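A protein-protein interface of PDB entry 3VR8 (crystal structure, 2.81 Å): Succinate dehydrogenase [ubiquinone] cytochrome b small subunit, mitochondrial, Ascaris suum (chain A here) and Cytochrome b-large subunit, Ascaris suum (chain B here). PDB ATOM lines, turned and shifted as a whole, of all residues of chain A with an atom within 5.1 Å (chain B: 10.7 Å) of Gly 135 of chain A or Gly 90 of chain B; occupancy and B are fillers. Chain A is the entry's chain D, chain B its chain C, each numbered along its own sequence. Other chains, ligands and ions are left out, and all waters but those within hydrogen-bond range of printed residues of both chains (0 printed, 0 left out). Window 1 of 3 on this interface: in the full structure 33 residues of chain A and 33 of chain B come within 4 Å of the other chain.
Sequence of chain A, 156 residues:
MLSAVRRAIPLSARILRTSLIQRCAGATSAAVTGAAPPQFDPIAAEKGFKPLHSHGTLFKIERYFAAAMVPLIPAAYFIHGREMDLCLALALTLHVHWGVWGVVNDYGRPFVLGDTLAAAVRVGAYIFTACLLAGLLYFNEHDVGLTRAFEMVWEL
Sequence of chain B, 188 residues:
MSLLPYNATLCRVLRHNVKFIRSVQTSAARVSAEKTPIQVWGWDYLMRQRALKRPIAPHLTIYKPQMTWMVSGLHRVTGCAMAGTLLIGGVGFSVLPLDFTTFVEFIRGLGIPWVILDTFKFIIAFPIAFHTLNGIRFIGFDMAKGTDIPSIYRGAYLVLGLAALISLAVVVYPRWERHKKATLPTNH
O of Val 91 of chain B sits at hydrogen-bond distance from OG of Ser 94 of chain B. The backbone carbonyl oxygen of Gly 90 of chain B sits at hydrogen-bond distance from the side-chain hydroxyl of Ser 94 of chain B.
Val 91 of chain B touches Cys 131 of chain A. CD1 of Leu 132 of chain A touches C of Leu 86 of chain B, at 3.7 Å. N of Leu 87 of chain B touches CD1 of Leu 132 of chain A, 3.7 Å away. O of Gly 135 of chain A touches CA of Gly 90 of chain B (3.2 Å). Gly 135 of chain A touches Val 91 of chain B. CD1 of Leu 136 of chain A touches O of Leu 86 of chain B, at 3.5 Å. Tyr 138 of chain A touches Phe 93 of chain B. CE1 of Tyr 138 of chain A touches CA of Ser 94 of chain B, at 3.4 Å. Phe 100 of chain B touches Phe 139 of chain A (CG to CZ, 3.98 Å).
Gly 135 of chain A touches just these residues of chain B: Gly 90 and Val 91. Gly 90 of chain B touches just one residue of chain A: Gly 135 (3.2 Å). No residue of chain B comes within 4 Å of Ala 134 of chain A. Phe 139 of chain A touches one residue of chain B. Of the printed residues of chain B, Cys 131 of chain A touches Val 91 (3.8 Å). Printed residues of chain A within 4 Å of Val 91 of chain B: Cys 131 and Gly 135. Printed residues of chain A within 4 Å of Ser 94 of chain B: Tyr 138 (3.4 Å). Of the printed residues of chain A, Phe 93 of chain B touches Tyr 138 (3.5 Å). Of the printed residues of chain A, Phe 100 of chain B touches Phe 139 (3.98 Å). Pro 97 of chain B touches none of the printed residues of chain A. Thr 85 of chain B touches none of the printed residues of chain A. The nearest residue of chain B that does not touch Gly 135 of chain A is Ser 94 of chain B (4.5 Å).
Of the 20 printed residues of chain B, 7 touch a printed residue of chain A. Printed residues of chain B that touch a printed residue of chain A: Leu 86, Leu 87, Gly 90, Val 91, Phe 93, Ser 94 and Phe 100. Hydrophobic or aromatic side chains of chain B within 4 Å of the printed part of chain A: Leu 86, Leu 87, Val 91 and Phe 100. Hydrophobic or aromatic side chains of chain A within 4 Å of the printed part of chain B: Leu 132, Leu 136, Tyr 138 and Phe 139. Among the printed residues, 9 pairs touch across the chains.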
ATOM      1  N   CYS A 131     -12.914  10.272  28.858  1.00  0.00           N
ATOM      2  CA  CYS A 131     -14.009   9.363  28.539  1.00  0.00           C
ATOM      3  C   CYS A 131     -15.343  10.052  28.690  1.00  0.00           C
ATOM      4  O   CYS A 131     -16.328   9.626  28.063  1.00  0.00           O
ATOM      5  CB  CYS A 131     -13.999   8.135  29.431  1.00  0.00           C
ATOM      6  SG  CYS A 131     -12.443   7.293  29.354  1.00  0.00           S
ATOM      7  N   LEU A 132     -15.391  11.100  29.525  1.00  0.00           N
ATOM      8  CA  LEU A 132     -16.631  11.858  29.710  1.00  0.00           C
ATOM      9  C   LEU A 132     -17.095  12.377  28.352  1.00  0.00           C
ATOM     10  O   LEU A 132     -18.213  12.066  27.898  1.00  0.00           O
ATOM     11  CB  LEU A 132     -16.459  13.016  30.700  1.00  0.00           C
ATOM     12  CG  LEU A 132     -17.735  13.830  30.990  1.00  0.00           C
ATOM     13  CD1 LEU A 132     -18.703  13.005  31.858  1.00  0.00           C
ATOM     14  CD2 LEU A 132     -17.460  15.203  31.599  1.00  0.00           C
ATOM     15  N   LEU A 133     -16.208  13.138  27.704  1.00  0.00           N
ATOM     16  CA  LEU A 133     -16.501  13.748  26.408  1.00  0.00           C
ATOM     17  C   LEU A 133     -16.808  12.698  25.331  1.00  0.00           C
ATOM     18  O   LEU A 133     -17.882  12.740  24.723  1.00  0.00           O
ATOM     19  CB  LEU A 133     -15.370  14.691  25.974  1.00  0.00           C
ATOM     20  CG  LEU A 133     -15.561  15.542  24.719  1.00  0.00           C
ATOM     21  CD1 LEU A 133     -16.471  16.720  24.983  1.00  0.00           C
ATOM     22  CD2 LEU A 133     -14.211  16.028  24.281  1.00  0.00           C
ATOM     23  N   ALA A 134     -15.878  11.763  25.112  1.00  0.00           N
ATOM     24  CA  ALA A 134     -16.084  10.651  24.187  1.00  0.00           C
ATOM     25  C   ALA A 134     -17.506  10.175  24.303  1.00  0.00           C
ATOM     26  O   ALA A 134     -18.256  10.244  23.335  1.00  0.00           O
ATOM     27  CB  ALA A 134     -15.133   9.511  24.483  1.00  0.00           C
ATOM     28  N   GLY A 135     -17.874   9.746  25.512  1.00  0.00           N
ATOM     29  CA  GLY A 135     -19.216   9.241  25.830  1.00  0.00           C
ATOM     30  C   GLY A 135     -20.369  10.190  25.578  1.00  0.00           C
ATOM     31  O   GLY A 135     -21.380   9.796  25.017  1.00  0.00           O
ATOM     32  N   LEU A 136     -20.227  11.438  26.006  1.00  0.00           N
ATOM     33  CA  LEU A 136     -21.200  12.465  25.633  1.00  0.00           C
ATOM     34  C   LEU A 136     -21.252  12.676  24.118  1.00  0.00           C
ATOM     35  O   LEU A 136     -22.317  12.503  23.511  1.00  0.00           O
ATOM     36  CB  LEU A 136     -20.932  13.795  26.346  1.00  0.00           C
ATOM     37  CG  LEU A 136     -21.834  14.238  27.496  1.00  0.00           C
ATOM     38  CD1 LEU A 136     -22.422  13.073  28.266  1.00  0.00           C
ATOM     39  CD2 LEU A 136     -20.982  15.077  28.403  1.00  0.00           C
ATOM     40  N   LEU A 137     -20.122  13.039  23.509  1.00  0.00           N
ATOM     41  CA  LEU A 137     -20.087  13.212  22.077  1.00  0.00           C
ATOM     42  C   LEU A 137     -20.899  12.110  21.431  1.00  0.00           C
ATOM     43  O   LEU A 137     -21.919  12.353  20.789  1.00  0.00           O
ATOM     44  CB  LEU A 137     -18.669  13.148  21.570  1.00  0.00           C
ATOM     45  CG  LEU A 137     -17.864  14.424  21.710  1.00  0.00           C
ATOM     46  CD1 LEU A 137     -16.420  14.065  21.439  1.00  0.00           C
ATOM     47  CD2 LEU A 137     -18.352  15.466  20.738  1.00  0.00           C
ATOM     48  N   TYR A 138     -20.457  10.884  21.627  1.00  0.00           N
ATOM     49  CA  TYR A 138     -21.200   9.746  21.157  1.00  0.00           C
ATOM     50  C   TYR A 138     -22.726   9.910  21.319  1.00  0.00           C
ATOM     51  O   TYR A 138     -23.446   9.902  20.340  1.00  0.00           O
ATOM     52  CB  TYR A 138     -20.709   8.474  21.858  1.00  0.00           C
ATOM     53  CG  TYR A 138     -21.595   7.346  21.519  1.00  0.00           C
ATOM     54  CD1 TYR A 138     -22.690   7.022  22.334  1.00  0.00           C
ATOM     55  CD2 TYR A 138     -21.407   6.659  20.330  1.00  0.00           C
ATOM     56  CE1 TYR A 138     -23.554   6.008  21.976  1.00  0.00           C
ATOM     57  CE2 TYR A 138     -22.249   5.652  19.956  1.00  0.00           C
ATOM     58  CZ  TYR A 138     -23.318   5.319  20.779  1.00  0.00           C
ATOM     59  OH  TYR A 138     -24.132   4.292  20.374  1.00  0.00           O
ATOM     60  N   PHE A 139     -23.201  10.052  22.551  1.00  0.00           N
ATOM     61  CA  PHE A 139     -24.641  10.161  22.866  1.00  0.00           C
ATOM     62  C   PHE A 139     -25.360  11.286  22.102  1.00  0.00           C
ATOM     63  O   PHE A 139     -26.529  11.152  21.740  1.00  0.00           O
ATOM     64  CB  PHE A 139     -24.809  10.379  24.377  1.00  0.00           C
ATOM     65  CG  PHE A 139     -26.215  10.180  24.892  1.00  0.00           C
ATOM     66  CD1 PHE A 139     -26.654   8.921  25.286  1.00  0.00           C
ATOM     67  CD2 PHE A 139     -27.081  11.261  25.031  1.00  0.00           C
ATOM     68  CE1 PHE A 139     -27.942   8.730  25.785  1.00  0.00           C
ATOM     69  CE2 PHE A 139     -28.368  11.080  25.529  1.00  0.00           C
ATOM     70  CZ  PHE A 139     -28.797   9.810  25.904  1.00  0.00           C
ATOM     71  N   ALA B  81     -22.184  13.102  41.557  1.00  0.00           N
ATOM     72  CA  ALA B  81     -23.259  12.243  41.050  1.00  0.00           C
ATOM     73  C   ALA B  81     -23.686  12.568  39.607  1.00  0.00           C
ATOM     74  O   ALA B  81     -23.863  11.653  38.799  1.00  0.00           O
ATOM     75  CB  ALA B  81     -24.470  12.265  41.999  1.00  0.00           C
ATOM     76  N   MET B  82     -23.849  13.858  39.289  1.00  0.00           N
ATOM     77  CA  MET B  82     -24.172  14.289  37.928  1.00  0.00           C
ATOM     78  C   MET B  82     -23.045  13.867  37.022  1.00  0.00           C
ATOM     79  O   MET B  82     -23.262  13.124  36.078  1.00  0.00           O
ATOM     80  CB  MET B  82     -24.369  15.806  37.819  1.00  0.00           C
ATOM     81  CG  MET B  82     -25.608  16.359  38.532  1.00  0.00           C
ATOM     82  SD  MET B  82     -25.675  18.168  38.577  1.00  0.00           S
ATOM     83  CE  MET B  82     -24.284  18.613  39.605  1.00  0.00           C
ATOM     84  N   ALA B  83     -21.831  14.310  37.310  1.00  0.00           N
ATOM     85  CA  ALA B  83     -20.700  13.891  36.504  1.00  0.00           C
ATOM     86  C   ALA B  83     -20.685  12.361  36.348  1.00  0.00           C
ATOM     87  O   ALA B  83     -20.568  11.848  35.236  1.00  0.00           O
ATOM     88  CB  ALA B  83     -19.406  14.405  37.089  1.00  0.00           C
ATOM     89  N   GLY B  84     -20.854  11.636  37.449  1.00  0.00           N
ATOM     90  CA  GLY B  84     -20.895  10.188  37.404  1.00  0.00           C
ATOM     91  C   GLY B  84     -21.969   9.620  36.505  1.00  0.00           C
ATOM     92  O   GLY B  84     -21.767   8.583  35.899  1.00  0.00           O
ATOM     93  N   THR B  85     -23.120  10.274  36.437  1.00  0.00           N
ATOM     94  CA  THR B  85     -24.191   9.878  35.515  1.00  0.00           C
ATOM     95  C   THR B  85     -23.791  10.177  34.078  1.00  0.00           C
ATOM     96  O   THR B  85     -23.974   9.361  33.185  1.00  0.00           O
ATOM     97  CB  THR B  85     -25.512  10.629  35.825  1.00  0.00           C
ATOM     98  OG1 THR B  85     -26.259   9.907  36.808  1.00  0.00           O
ATOM     99  CG2 THR B  85     -26.373  10.790  34.573  1.00  0.00           C
ATOM    100  N   LEU B  86     -23.248  11.369  33.864  1.00  0.00           N
ATOM    101  CA  LEU B  86     -22.844  11.789  32.540  1.00  0.00           C
ATOM    102  C   LEU B  86     -21.756  10.885  31.945  1.00  0.00           C
ATOM    103  O   LEU B  86     -21.662  10.747  30.721  1.00  0.00           O
ATOM    104  CB  LEU B  86     -22.404  13.253  32.559  1.00  0.00           C
ATOM    105  CG  LEU B  86     -23.517  14.289  32.483  1.00  0.00           C
ATOM    106  CD1 LEU B  86     -22.929  15.641  32.138  1.00  0.00           C
ATOM    107  CD2 LEU B  86     -24.526  13.859  31.446  1.00  0.00           C
ATOM    108  N   LEU B  87     -20.937  10.275  32.801  1.00  0.00           N
ATOM    109  CA  LEU B  87     -20.105   9.154  32.362  1.00  0.00           C
ATOM    110  C   LEU B  87     -20.969   7.915  32.121  1.00  0.00           C
ATOM    111  O   LEU B  87     -21.364   7.698  30.988  1.00  0.00           O
ATOM    112  CB  LEU B  87     -18.962   8.849  33.315  1.00  0.00           C
ATOM    113  CG  LEU B  87     -17.869   8.102  32.562  1.00  0.00           C
ATOM    114  CD1 LEU B  87     -16.625   8.981  32.460  1.00  0.00           C
ATOM    115  CD2 LEU B  87     -17.566   6.717  33.197  1.00  0.00           C
ATOM    116  N   ILE B  88     -21.299   7.127  33.152  1.00  0.00           N
ATOM    117  CA  ILE B  88     -22.053   5.862  32.932  1.00  0.00           C
ATOM    118  C   ILE B  88     -23.193   6.016  31.893  1.00  0.00           C
ATOM    119  O   ILE B  88     -23.627   5.046  31.275  1.00  0.00           O
ATOM    120  CB  ILE B  88     -22.526   5.121  34.270  1.00  0.00           C
ATOM    121  CG1 ILE B  88     -23.766   5.776  34.908  1.00  0.00           C
ATOM    122  CG2 ILE B  88     -21.389   5.012  35.298  1.00  0.00           C
ATOM    123  CD1 ILE B  88     -25.156   5.148  34.536  1.00  0.00           C
ATOM    124  N   GLY B  89     -23.657   7.248  31.705  1.00  0.00           N
ATOM    125  CA  GLY B  89     -24.683   7.552  30.717  1.00  0.00           C
ATOM    126  C   GLY B  89     -24.085   7.453  29.339  1.00  0.00           C
ATOM    127  O   GLY B  89     -24.251   6.448  28.676  1.00  0.00           O
ATOM    128  N   GLY B  90     -23.366   8.492  28.928  1.00  0.00           N
ATOM    129  CA  GLY B  90     -22.655   8.505  27.650  1.00  0.00           C
ATOM    130  C   GLY B  90     -21.893   7.234  27.312  1.00  0.00           C
ATOM    131  O   GLY B  90     -22.277   6.495  26.405  1.00  0.00           O
ATOM    132  N   VAL B  91     -20.809   6.979  28.035  1.00  0.00           N
ATOM    133  CA  VAL B  91     -20.045   5.755  27.839  1.00  0.00           C
ATOM    134  C   VAL B  91     -20.882   4.456  27.925  1.00  0.00           C
ATOM    135  O   VAL B  91     -20.731   3.573  27.081  1.00  0.00           O
ATOM    136  CB  VAL B  91     -18.760   5.727  28.712  1.00  0.00           C
ATOM    137  CG1 VAL B  91     -18.606   4.413  29.484  1.00  0.00           C
ATOM    138  CG2 VAL B  91     -17.541   5.997  27.844  1.00  0.00           C
ATOM    139  N   GLY B  92     -21.774   4.338  28.903  1.00  0.00           N
ATOM    140  CA  GLY B  92     -22.553   3.107  29.031  1.00  0.00           C
ATOM    141  C   GLY B  92     -23.509   2.795  27.881  1.00  0.00           C
ATOM    142  O   GLY B  92     -23.816   1.629  27.628  1.00  0.00           O
ATOM    143  N   PHE B  93     -23.985   3.832  27.196  1.00  0.00           N
ATOM    144  CA  PHE B  93     -24.979   3.677  26.132  1.00  0.00           C
ATOM    145  C   PHE B  93     -24.285   3.594  24.785  1.00  0.00           C
ATOM    146  O   PHE B  93     -24.927   3.329  23.768  1.00  0.00           O
ATOM    147  CB  PHE B  93     -26.017   4.812  26.151  1.00  0.00           C
ATOM    148  CG  PHE B  93     -27.062   4.680  27.242  1.00  0.00           C
ATOM    149  CD1 PHE B  93     -26.702   4.374  28.561  1.00  0.00           C
ATOM    150  CD2 PHE B  93     -28.403   4.880  26.960  1.00  0.00           C
ATOM    151  CE1 PHE B  93     -27.669   4.256  29.576  1.00  0.00           C
ATOM    152  CE2 PHE B  93     -29.370   4.763  27.964  1.00  0.00           C
ATOM    153  CZ  PHE B  93     -29.002   4.455  29.267  1.00  0.00           C
ATOM    154  N   SER B  94     -22.972   3.833  24.790  1.00  0.00           N
ATOM    155  CA  SER B  94     -22.099   3.451  23.669  1.00  0.00           C
ATOM    156  C   SER B  94     -21.674   1.998  23.815  1.00  0.00           C
ATOM    157  O   SER B  94     -22.130   1.137  23.064  1.00  0.00           O
ATOM    158  CB  SER B  94     -20.871   4.368  23.526  1.00  0.00           C
ATOM    159  OG  SER B  94     -20.552   5.034  24.732  1.00  0.00           O
ATOM    160  N   VAL B  95     -20.829   1.732  24.806  1.00  0.00           N
ATOM    161  CA  VAL B  95     -20.317   0.387  25.082  1.00  0.00           C
ATOM    162  C   VAL B  95     -21.412  -0.712  25.201  1.00  0.00           C
ATOM    163  O   VAL B  95     -21.110  -1.904  25.213  1.00  0.00           O
ATOM    164  CB  VAL B  95     -19.303   0.443  26.275  1.00  0.00           C
ATOM    165  CG1 VAL B  95     -19.103  -0.913  26.973  1.00  0.00           C
ATOM    166  CG2 VAL B  95     -17.971   1.014  25.781  1.00  0.00           C
ATOM    167  N   LEU B  96     -22.678  -0.314  25.235  1.00  0.00           N
ATOM    168  CA  LEU B  96     -23.773  -1.279  25.290  1.00  0.00           C
ATOM    169  C   LEU B  96     -24.713  -1.157  24.086  1.00  0.00           C
ATOM    170  O   LEU B  96     -24.811  -0.069  23.486  1.00  0.00           O
ATOM    171  CB  LEU B  96     -24.585  -1.081  26.576  1.00  0.00           C
ATOM    172  CG  LEU B  96     -24.396  -1.988  27.795  1.00  0.00           C
ATOM    173  CD1 LEU B  96     -23.219  -1.543  28.667  1.00  0.00           C
ATOM    174  CD2 LEU B  96     -25.697  -2.007  28.603  1.00  0.00           C
ATOM    175  N   PRO B  97     -25.413  -2.271  23.735  1.00  0.00           N
ATOM    176  CA  PRO B  97     -26.572  -2.273  22.809  1.00  0.00           C
ATOM    177  C   PRO B  97     -27.743  -1.416  23.343  1.00  0.00           C
ATOM    178  O   PRO B  97     -27.716  -0.183  23.184  1.00  0.00           O
ATOM    179  CB  PRO B  97     -26.963  -3.758  22.733  1.00  0.00           C
ATOM    180  CG  PRO B  97     -26.350  -4.387  23.963  1.00  0.00           C
ATOM    181  CD  PRO B  97     -25.068  -3.639  24.172  1.00  0.00           C
ATOM    182  N   LEU B  98     -28.750  -2.071  23.942  1.00  0.00           N
ATOM    183  CA  LEU B  98     -29.816  -1.439  24.766  1.00  0.00           C
ATOM    184  C   LEU B  98     -29.737   0.104  24.854  1.00  0.00           C
ATOM    185  O   LEU B  98     -29.287   0.623  25.872  1.00  0.00           O
ATOM    186  CB  LEU B  98     -29.771  -2.027  26.208  1.00  0.00           C
ATOM    187  CG  LEU B  98     -30.187  -3.423  26.791  1.00  0.00           C
ATOM    188  CD1 LEU B  98     -30.599  -4.551  25.801  1.00  0.00           C
ATOM    189  CD2 LEU B  98     -29.136  -3.963  27.818  1.00  0.00           C
ATOM    190  N   ASP B  99     -30.153   0.830  23.808  1.00  0.00           N
ATOM    191  CA  ASP B  99     -29.993   2.301  23.772  1.00  0.00           C
ATOM    192  C   ASP B  99     -31.065   3.051  24.608  1.00  0.00           C
ATOM    193  O   ASP B  99     -31.926   2.406  25.219  1.00  0.00           O
ATOM    194  CB  ASP B  99     -29.904   2.803  22.324  1.00  0.00           C
ATOM    195  CG  ASP B  99     -31.255   3.214  21.746  1.00  0.00           C
ATOM    196  OD1 ASP B  99     -31.692   4.361  21.998  1.00  0.00           O
ATOM    197  OD2 ASP B  99     -31.872   2.405  21.018  1.00  0.00           O
ATOM    198  N   PHE B 100     -31.005   4.391  24.634  1.00  0.00           N
ATOM    199  CA  PHE B 100     -31.868   5.237  25.502  1.00  0.00           C
ATOM    200  C   PHE B 100     -33.362   5.209  25.164  1.00  0.00           C
ATOM    201  O   PHE B 100     -34.196   5.176  26.065  1.00  0.00           O
ATOM    202  CB  PHE B 100     -31.359   6.693  25.533  1.00  0.00           C
ATOM    203  CG  PHE B 100     -32.006   7.568  26.599  1.00  0.00           C
ATOM    204  CD1 PHE B 100     -32.916   8.558  26.252  1.00  0.00           C
ATOM    205  CD2 PHE B 100     -31.684   7.425  27.943  1.00  0.00           C
ATOM    206  CE1 PHE B 100     -33.505   9.373  27.228  1.00  0.00           C
ATOM    207  CE2 PHE B 100     -32.285   8.245  28.916  1.00  0.00           C
ATOM    208  CZ  PHE B 100     -33.184   9.218  28.547  1.00  0.00           C
